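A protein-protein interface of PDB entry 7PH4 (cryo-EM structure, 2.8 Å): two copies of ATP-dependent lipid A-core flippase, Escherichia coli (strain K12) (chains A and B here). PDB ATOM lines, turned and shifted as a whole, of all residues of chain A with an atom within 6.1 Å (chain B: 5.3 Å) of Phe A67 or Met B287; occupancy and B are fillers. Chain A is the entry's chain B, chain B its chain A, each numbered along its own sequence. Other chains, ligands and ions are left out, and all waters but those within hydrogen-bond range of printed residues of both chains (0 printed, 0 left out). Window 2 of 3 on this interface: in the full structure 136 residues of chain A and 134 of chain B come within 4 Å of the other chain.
SD of Met B287 sits close to O of Phe A67 (3.6 Å).
The backbone carbonyl oxygen (O) of Ser B282 is in hydrogen-bond range of the guanidinium group (NH2) of Arg A72.
Among the printed residues, pairs that only touch across the chains: Arg A72 with Pro B284 (3.4 Å), Arg A72 with Met B287 (3.5 Å), Phe A67 with Thr B291 (3.6 Å), Leu A63 with Ala B292 (3.6 Å), Leu A75 with Ser B282 (3.7 Å), Phe A67 with Ala B292 (3.7 Å), Phe A67 with Ile B295 (3.9 Å) and Leu A75 with Ala B281 (3.9 Å).
Phe A67 touches just these residues of chain B: Met B287 (3.2 Å), Thr B291 (3.6 Å), Ala B292 (3.7 Å) and Ile B295 (3.9 Å).
Of chain A, only Phe A67 (3.2 Å) and Arg A72 (3.5 Å) come within 4 Å of Met B287.
Of the printed residues of chain A, Thr B291 touches Phe A67.
Of the printed residues of chain B, Leu A75 touches Ala B281 (3.9 Å) and Ser B282 (3.7 Å).
Printed residues of chain A within 4 Å of Ile B295: Phe A67.
Asp B288 touches none of the printed residues of chain A.
Ser B285 touches none of the printed residues of chain A.
The nearest residue of chain B that does not touch Phe A67 is Leu B290 (4.3 Å).
Of the 11 printed residues of chain A, 4 touch a printed residue of chain B.
Printed residues of chain A that touch a printed residue of chain B: Leu A63, Phe A67, Arg A72 and Leu A75.
Hydrophobic or aromatic side chains of chain A that line the printed part of chain B: Leu A63, Phe A67 and Leu A75.
Of the 13 printed residues of chain B, 7 touch a printed residue of chain A.
Hydrophobic or aromatic side chains of chain B within 4 Å of the printed part of chain A: Pro B284, Met B287, Ala B292 and Ile B295.
Along chain B the printed residues that touch a printed residue of chain A span positions 281 to 295.
No position is printed for both chains.
Of the 10 pairs that touch across the chains among the printed residues, none has its exchanged pair printed and touching as well.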
ATOM      1  N   LEU A  62     -35.082  -9.295  -2.017  1.00  0.00           N
ATOM      2  CA  LEU A  62     -33.684  -9.450  -2.404  1.00  0.00           C
ATOM      3  C   LEU A  62     -33.005  -8.103  -2.573  1.00  0.00           C
ATOM      4  O   LEU A  62     -31.814  -7.958  -2.277  1.00  0.00           O
ATOM      5  CB  LEU A  62     -33.592 -10.256  -3.694  1.00  0.00           C
ATOM      6  CG  LEU A  62     -32.256 -10.260  -4.424  1.00  0.00           C
ATOM      7  CD1 LEU A  62     -31.267 -11.124  -3.686  1.00  0.00           C
ATOM      8  CD2 LEU A  62     -32.430 -10.743  -5.845  1.00  0.00           C
ATOM      9  N   LEU A  63     -33.743  -7.106  -3.042  1.00  0.00           N
ATOM     10  CA  LEU A  63     -33.198  -5.787  -3.313  1.00  0.00           C
ATOM     11  C   LEU A  63     -33.365  -4.847  -2.126  1.00  0.00           C
ATOM     12  O   LEU A  63     -32.386  -4.266  -1.652  1.00  0.00           O
ATOM     13  CB  LEU A  63     -33.873  -5.200  -4.547  1.00  0.00           C
ATOM     14  CG  LEU A  63     -33.438  -3.793  -4.903  1.00  0.00           C
ATOM     15  CD1 LEU A  63     -31.972  -3.803  -5.235  1.00  0.00           C
ATOM     16  CD2 LEU A  63     -34.253  -3.289  -6.072  1.00  0.00           C
ATOM     17  N   ASP A  65     -34.301  -5.499   1.189  1.00  0.00           N
ATOM     18  CA  ASP A  65     -33.436  -6.135   2.178  1.00  0.00           C
ATOM     19  C   ASP A  65     -32.161  -6.519   1.437  1.00  0.00           C
ATOM     20  O   ASP A  65     -31.972  -7.658   1.003  1.00  0.00           O
ATOM     21  CB  ASP A  65     -34.126  -7.340   2.813  1.00  0.00           C
ATOM     22  CG  ASP A  65     -33.284  -8.015   3.885  1.00  0.00           C
ATOM     23  OD1 ASP A  65     -32.079  -8.257   3.662  1.00  0.00           O
ATOM     24  OD2 ASP A  65     -33.836  -8.318   4.962  1.00  0.00           O
ATOM     25  N   GLY A  66     -31.278  -5.537   1.288  1.00  0.00           N
ATOM     26  CA  GLY A  66     -30.133  -5.668   0.406  1.00  0.00           C
ATOM     27  C   GLY A  66     -29.269  -6.871   0.734  1.00  0.00           C
ATOM     28  O   GLY A  66     -29.314  -7.451   1.819  1.00  0.00           O
ATOM     29  N   PHE A  67     -28.463  -7.257  -0.256  1.00  0.00           N
ATOM     30  CA  PHE A  67     -27.591  -8.413  -0.087  1.00  0.00           C
ATOM     31  C   PHE A  67     -26.580  -8.185   1.029  1.00  0.00           C
ATOM     32  O   PHE A  67     -26.286  -9.100   1.809  1.00  0.00           O
ATOM     33  CB  PHE A  67     -26.885  -8.733  -1.405  1.00  0.00           C
ATOM     34  CG  PHE A  67     -26.544  -7.519  -2.224  1.00  0.00           C
ATOM     35  CD1 PHE A  67     -25.375  -6.813  -1.992  1.00  0.00           C
ATOM     36  CD2 PHE A  67     -27.389  -7.089  -3.234  1.00  0.00           C
ATOM     37  CE1 PHE A  67     -25.057  -5.698  -2.748  1.00  0.00           C
ATOM     38  CE2 PHE A  67     -27.079  -5.975  -3.992  1.00  0.00           C
ATOM     39  CZ  PHE A  67     -25.911  -5.281  -3.751  1.00  0.00           C
ATOM     40  N   GLY A  68     -26.043  -6.973   1.129  1.00  0.00           N
ATOM     41  CA  GLY A  68     -25.111  -6.648   2.189  1.00  0.00           C
ATOM     42  C   GLY A  68     -25.583  -5.488   3.040  1.00  0.00           C
ATOM     43  O   GLY A  68     -25.117  -5.307   4.169  1.00  0.00           O
ATOM     44  N   LYS A  69     -26.512  -4.692   2.504  1.00  0.00           N
ATOM     45  CA  LYS A  69     -27.028  -3.551   3.253  1.00  0.00           C
ATOM     46  C   LYS A  69     -27.751  -4.001   4.513  1.00  0.00           C
ATOM     47  O   LYS A  69     -27.583  -3.404   5.583  1.00  0.00           O
ATOM     48  CB  LYS A  69     -27.962  -2.723   2.372  1.00  0.00           C
ATOM     49  CG  LYS A  69     -28.591  -1.543   3.093  1.00  0.00           C
ATOM     50  CD  LYS A  69     -29.503  -0.755   2.173  1.00  0.00           C
ATOM     51  CE  LYS A  69     -30.668  -1.599   1.696  1.00  0.00           C
ATOM     52  NZ  LYS A  69     -31.553  -0.842   0.771  1.00  0.00           N
ATOM     53  N   THR A  70     -28.555  -5.049   4.410  1.00  0.00           N
ATOM     54  CA  THR A  70     -29.323  -5.570   5.529  1.00  0.00           C
ATOM     55  C   THR A  70     -28.806  -6.966   5.877  1.00  0.00           C
ATOM     56  O   THR A  70     -27.803  -7.433   5.330  1.00  0.00           O
ATOM     57  CB  THR A  70     -30.816  -5.578   5.194  1.00  0.00           C
ATOM     58  OG1 THR A  70     -31.168  -4.340   4.567  1.00  0.00           O
ATOM     59  CG2 THR A  70     -31.642  -5.742   6.460  1.00  0.00           C
ATOM     60  N   ASP A  71     -29.496  -7.626   6.802  1.00  0.00           N
ATOM     61  CA  ASP A  71     -29.085  -8.953   7.233  1.00  0.00           C
ATOM     62  C   ASP A  71     -29.186  -9.953   6.090  1.00  0.00           C
ATOM     63  O   ASP A  71     -30.102  -9.905   5.265  1.00  0.00           O
ATOM     64  CB  ASP A  71     -29.941  -9.423   8.408  1.00  0.00           C
ATOM     65  CG  ASP A  71     -29.775  -8.549   9.631  1.00  0.00           C
ATOM     66  OD1 ASP A  71     -29.000  -7.573   9.563  1.00  0.00           O
ATOM     67  OD2 ASP A  71     -30.419  -8.838  10.660  1.00  0.00           O
ATOM     68  N   ARG A  72     -28.251 -10.899   6.052  1.00  0.00           N
ATOM     69  CA  ARG A  72     -28.252 -11.910   4.968  1.00  0.00           C
ATOM     70  C   ARG A  72     -29.284 -13.001   5.272  1.00  0.00           C
ATOM     71  O   ARG A  72     -29.359 -13.948   4.474  1.00  0.00           O
ATOM     72  CB  ARG A  72     -26.849 -12.495   4.802  1.00  0.00           C
ATOM     73  CG  ARG A  72     -26.206 -12.956   6.101  1.00  0.00           C
ATOM     74  CD  ARG A  72     -24.802 -13.442   5.812  1.00  0.00           C
ATOM     75  NE  ARG A  72     -24.073 -12.443   5.045  1.00  0.00           N
ATOM     76  CZ  ARG A  72     -22.893 -12.644   4.474  1.00  0.00           C
ATOM     77  NH1 ARG A  72     -22.313 -11.668   3.797  1.00  0.00           N
ATOM     78  NH2 ARG A  72     -22.302 -13.821   4.572  1.00  0.00           N
ATOM     79  N   LEU A  75     -30.927 -14.211   2.226  1.00  0.00           N
ATOM     80  CA  LEU A  75     -30.117 -15.002   1.310  1.00  0.00           C
ATOM     81  C   LEU A  75     -29.672 -16.319   1.923  1.00  0.00           C
ATOM     82  O   LEU A  75     -29.182 -17.191   1.200  1.00  0.00           O
ATOM     83  CB  LEU A  75     -28.897 -14.210   0.858  1.00  0.00           C
ATOM     84  CG  LEU A  75     -29.199 -12.967   0.028  1.00  0.00           C
ATOM     85  CD1 LEU A  75     -27.967 -12.542  -0.752  1.00  0.00           C
ATOM     86  CD2 LEU A  75     -30.363 -13.224  -0.901  1.00  0.00           C
ATOM     87  N   ALA B 281     -24.362 -14.905  -4.474  1.00  0.00           N
ATOM     88  CA  ALA B 281     -24.528 -13.549  -3.966  1.00  0.00           C
ATOM     89  C   ALA B 281     -24.579 -13.541  -2.446  1.00  0.00           C
ATOM     90  O   ALA B 281     -24.228 -12.541  -1.813  1.00  0.00           O
ATOM     91  CB  ALA B 281     -25.787 -12.910  -4.553  1.00  0.00           C
ATOM     92  N   SER B 282     -25.008 -14.649  -1.839  1.00  0.00           N
ATOM     93  CA  SER B 282     -25.001 -14.729  -0.384  1.00  0.00           C
ATOM     94  C   SER B 282     -23.597 -14.638   0.193  1.00  0.00           C
ATOM     95  O   SER B 282     -23.448 -14.355   1.385  1.00  0.00           O
ATOM     96  CB  SER B 282     -25.652 -16.026   0.084  1.00  0.00           C
ATOM     97  OG  SER B 282     -24.730 -17.097   0.002  1.00  0.00           O
ATOM     98  N   PHE B 283     -22.568 -14.884  -0.609  1.00  0.00           N
ATOM     99  CA  PHE B 283     -21.206 -14.746  -0.120  1.00  0.00           C
ATOM    100  C   PHE B 283     -20.836 -13.270   0.011  1.00  0.00           C
ATOM    101  O   PHE B 283     -21.269 -12.446  -0.799  1.00  0.00           O
ATOM    102  CB  PHE B 283     -20.220 -15.449  -1.048  1.00  0.00           C
ATOM    103  CG  PHE B 283     -19.945 -16.870  -0.665  1.00  0.00           C
ATOM    104  CD1 PHE B 283     -20.573 -17.432   0.432  1.00  0.00           C
ATOM    105  CD2 PHE B 283     -19.052 -17.638  -1.388  1.00  0.00           C
ATOM    106  CE1 PHE B 283     -20.324 -18.733   0.794  1.00  0.00           C
ATOM    107  CE2 PHE B 283     -18.798 -18.942  -1.027  1.00  0.00           C
ATOM    108  CZ  PHE B 283     -19.436 -19.490   0.067  1.00  0.00           C
ATOM    109  N   PRO B 284     -20.043 -12.908   1.020  1.00  0.00           N
ATOM    110  CA  PRO B 284     -19.563 -11.527   1.137  1.00  0.00           C
ATOM    111  C   PRO B 284     -18.367 -11.216   0.255  1.00  0.00           C
ATOM    112  O   PRO B 284     -18.131 -10.041  -0.044  1.00  0.00           O
ATOM    113  CB  PRO B 284     -19.182 -11.434   2.618  1.00  0.00           C
ATOM    114  CG  PRO B 284     -18.720 -12.813   2.945  1.00  0.00           C
ATOM    115  CD  PRO B 284     -19.594 -13.747   2.144  1.00  0.00           C
ATOM    116  N   SER B 285     -17.621 -12.228  -0.179  1.00  0.00           N
ATOM    117  CA  SER B 285     -16.447 -12.033  -1.013  1.00  0.00           C
ATOM    118  C   SER B 285     -16.796 -11.705  -2.457  1.00  0.00           C
ATOM    119  O   SER B 285     -15.935 -11.212  -3.191  1.00  0.00           O
ATOM    120  CB  SER B 285     -15.563 -13.283  -0.970  1.00  0.00           C
ATOM    121  OG  SER B 285     -14.577 -13.238  -1.984  1.00  0.00           O
ATOM    122  N   VAL B 286     -18.029 -11.959  -2.879  1.00  0.00           N
ATOM    123  CA  VAL B 286     -18.477 -11.624  -4.220  1.00  0.00           C
ATOM    124  C   VAL B 286     -19.206 -10.288  -4.245  1.00  0.00           C
ATOM    125  O   VAL B 286     -19.047  -9.510  -5.185  1.00  0.00           O
ATOM    126  CB  VAL B 286     -19.365 -12.750  -4.785  1.00  0.00           C
ATOM    127  CG1 VAL B 286     -19.778 -12.427  -6.213  1.00  0.00           C
ATOM    128  CG2 VAL B 286     -18.636 -14.081  -4.719  1.00  0.00           C
ATOM    129  N   MET B 287     -20.002 -10.009  -3.219  1.00  0.00           N
ATOM    130  CA  MET B 287     -20.669  -8.724  -3.139  1.00  0.00           C
ATOM    131  C   MET B 287     -19.646  -7.622  -2.890  1.00  0.00           C
ATOM    132  O   MET B 287     -18.461  -7.873  -2.652  1.00  0.00           O
ATOM    133  CB  MET B 287     -21.739  -8.737  -2.051  1.00  0.00           C
ATOM    134  CG  MET B 287     -22.645  -9.946  -2.101  1.00  0.00           C
ATOM    135  SD  MET B 287     -23.956  -9.903  -0.862  1.00  0.00           S
ATOM    136  CE  MET B 287     -23.070 -10.326   0.640  1.00  0.00           C
ATOM    137  N   ASP B 288     -20.120  -6.379  -2.970  1.00  0.00           N
ATOM    138  CA  ASP B 288     -19.336  -5.151  -2.906  1.00  0.00           C
ATOM    139  C   ASP B 288     -18.445  -4.988  -4.126  1.00  0.00           C
ATOM    140  O   ASP B 288     -17.801  -3.942  -4.273  1.00  0.00           O
ATOM    141  CB  ASP B 288     -18.483  -5.057  -1.634  1.00  0.00           C
ATOM    142  CG  ASP B 288     -19.269  -5.390  -0.384  1.00  0.00           C
ATOM    143  OD1 ASP B 288     -20.466  -5.725  -0.506  1.00  0.00           O
ATOM    144  OD2 ASP B 288     -18.689  -5.320   0.720  1.00  0.00           O
ATOM    145  N   SER B 289     -18.384  -5.984  -5.010  1.00  0.00           N
ATOM    146  CA  SER B 289     -17.733  -5.804  -6.298  1.00  0.00           C
ATOM    147  C   SER B 289     -18.682  -5.197  -7.319  1.00  0.00           C
ATOM    148  O   SER B 289     -18.232  -4.543  -8.266  1.00  0.00           O
ATOM    149  CB  SER B 289     -17.195  -7.140  -6.810  1.00  0.00           C
ATOM    150  OG  SER B 289     -16.550  -6.979  -8.060  1.00  0.00           O
ATOM    151  N   LEU B 290     -19.987  -5.399  -7.142  1.00  0.00           N
ATOM    152  CA  LEU B 290     -20.994  -4.876  -8.051  1.00  0.00           C
ATOM    153  C   LEU B 290     -22.146  -4.300  -7.241  1.00  0.00           C
ATOM    154  O   LEU B 290     -22.360  -4.656  -6.080  1.00  0.00           O
ATOM    155  CB  LEU B 290     -21.491  -5.958  -9.014  1.00  0.00           C
ATOM    156  CG  LEU B 290     -20.432  -6.491  -9.977  1.00  0.00           C
ATOM    157  CD1 LEU B 290     -20.971  -7.647 -10.798  1.00  0.00           C
ATOM    158  CD2 LEU B 290     -19.930  -5.371 -10.876  1.00  0.00           C
ATOM    159  N   THR B 291     -22.895  -3.409  -7.875  1.00  0.00           N
ATOM    160  CA  THR B 291     -23.924  -2.636  -7.193  1.00  0.00           C
ATOM    161  C   THR B 291     -25.183  -3.480  -7.012  1.00  0.00           C
ATOM    162  O   THR B 291     -25.186  -4.699  -7.193  1.00  0.00           O
ATOM    163  CB  THR B 291     -24.210  -1.357  -7.974  1.00  0.00           C
ATOM    164  OG1 THR B 291     -24.642  -1.691  -9.299  1.00  0.00           O
ATOM    165  CG2 THR B 291     -22.963  -0.492  -8.051  1.00  0.00           C
ATOM    166  N   ALA B 292     -26.279  -2.824  -6.632  1.00  0.00           N
ATOM    167  CA  ALA B 292     -27.603  -3.442  -6.655  1.00  0.00           C
ATOM    168  C   ALA B 292     -28.134  -3.563  -8.071  1.00  0.00           C
ATOM    169  O   ALA B 292     -29.164  -4.193  -8.324  1.00  0.00           O
ATOM    170  CB  ALA B 292     -28.560  -2.638  -5.780  1.00  0.00           C
ATOM    171  N   ILE B 295     -26.955  -6.478 -10.514  1.00  0.00           N
ATOM    172  CA  ILE B 295     -27.665  -7.770 -10.210  1.00  0.00           C
ATOM    173  C   ILE B 295     -29.152  -7.611 -10.535  1.00  0.00           C
ATOM    174  O   ILE B 295     -29.839  -8.593 -10.802  1.00  0.00           O
ATOM    175  CB  ILE B 295     -27.411  -8.366  -8.814  1.00  0.00           C
ATOM    176  CG1 ILE B 295     -27.817  -7.401  -7.698  1.00  0.00           C
ATOM    177  CG2 ILE B 295     -25.964  -8.805  -8.673  1.00  0.00           C
ATOM    178  CD1 ILE B 295     -28.903  -7.934  -6.794  1.00  0.00           C
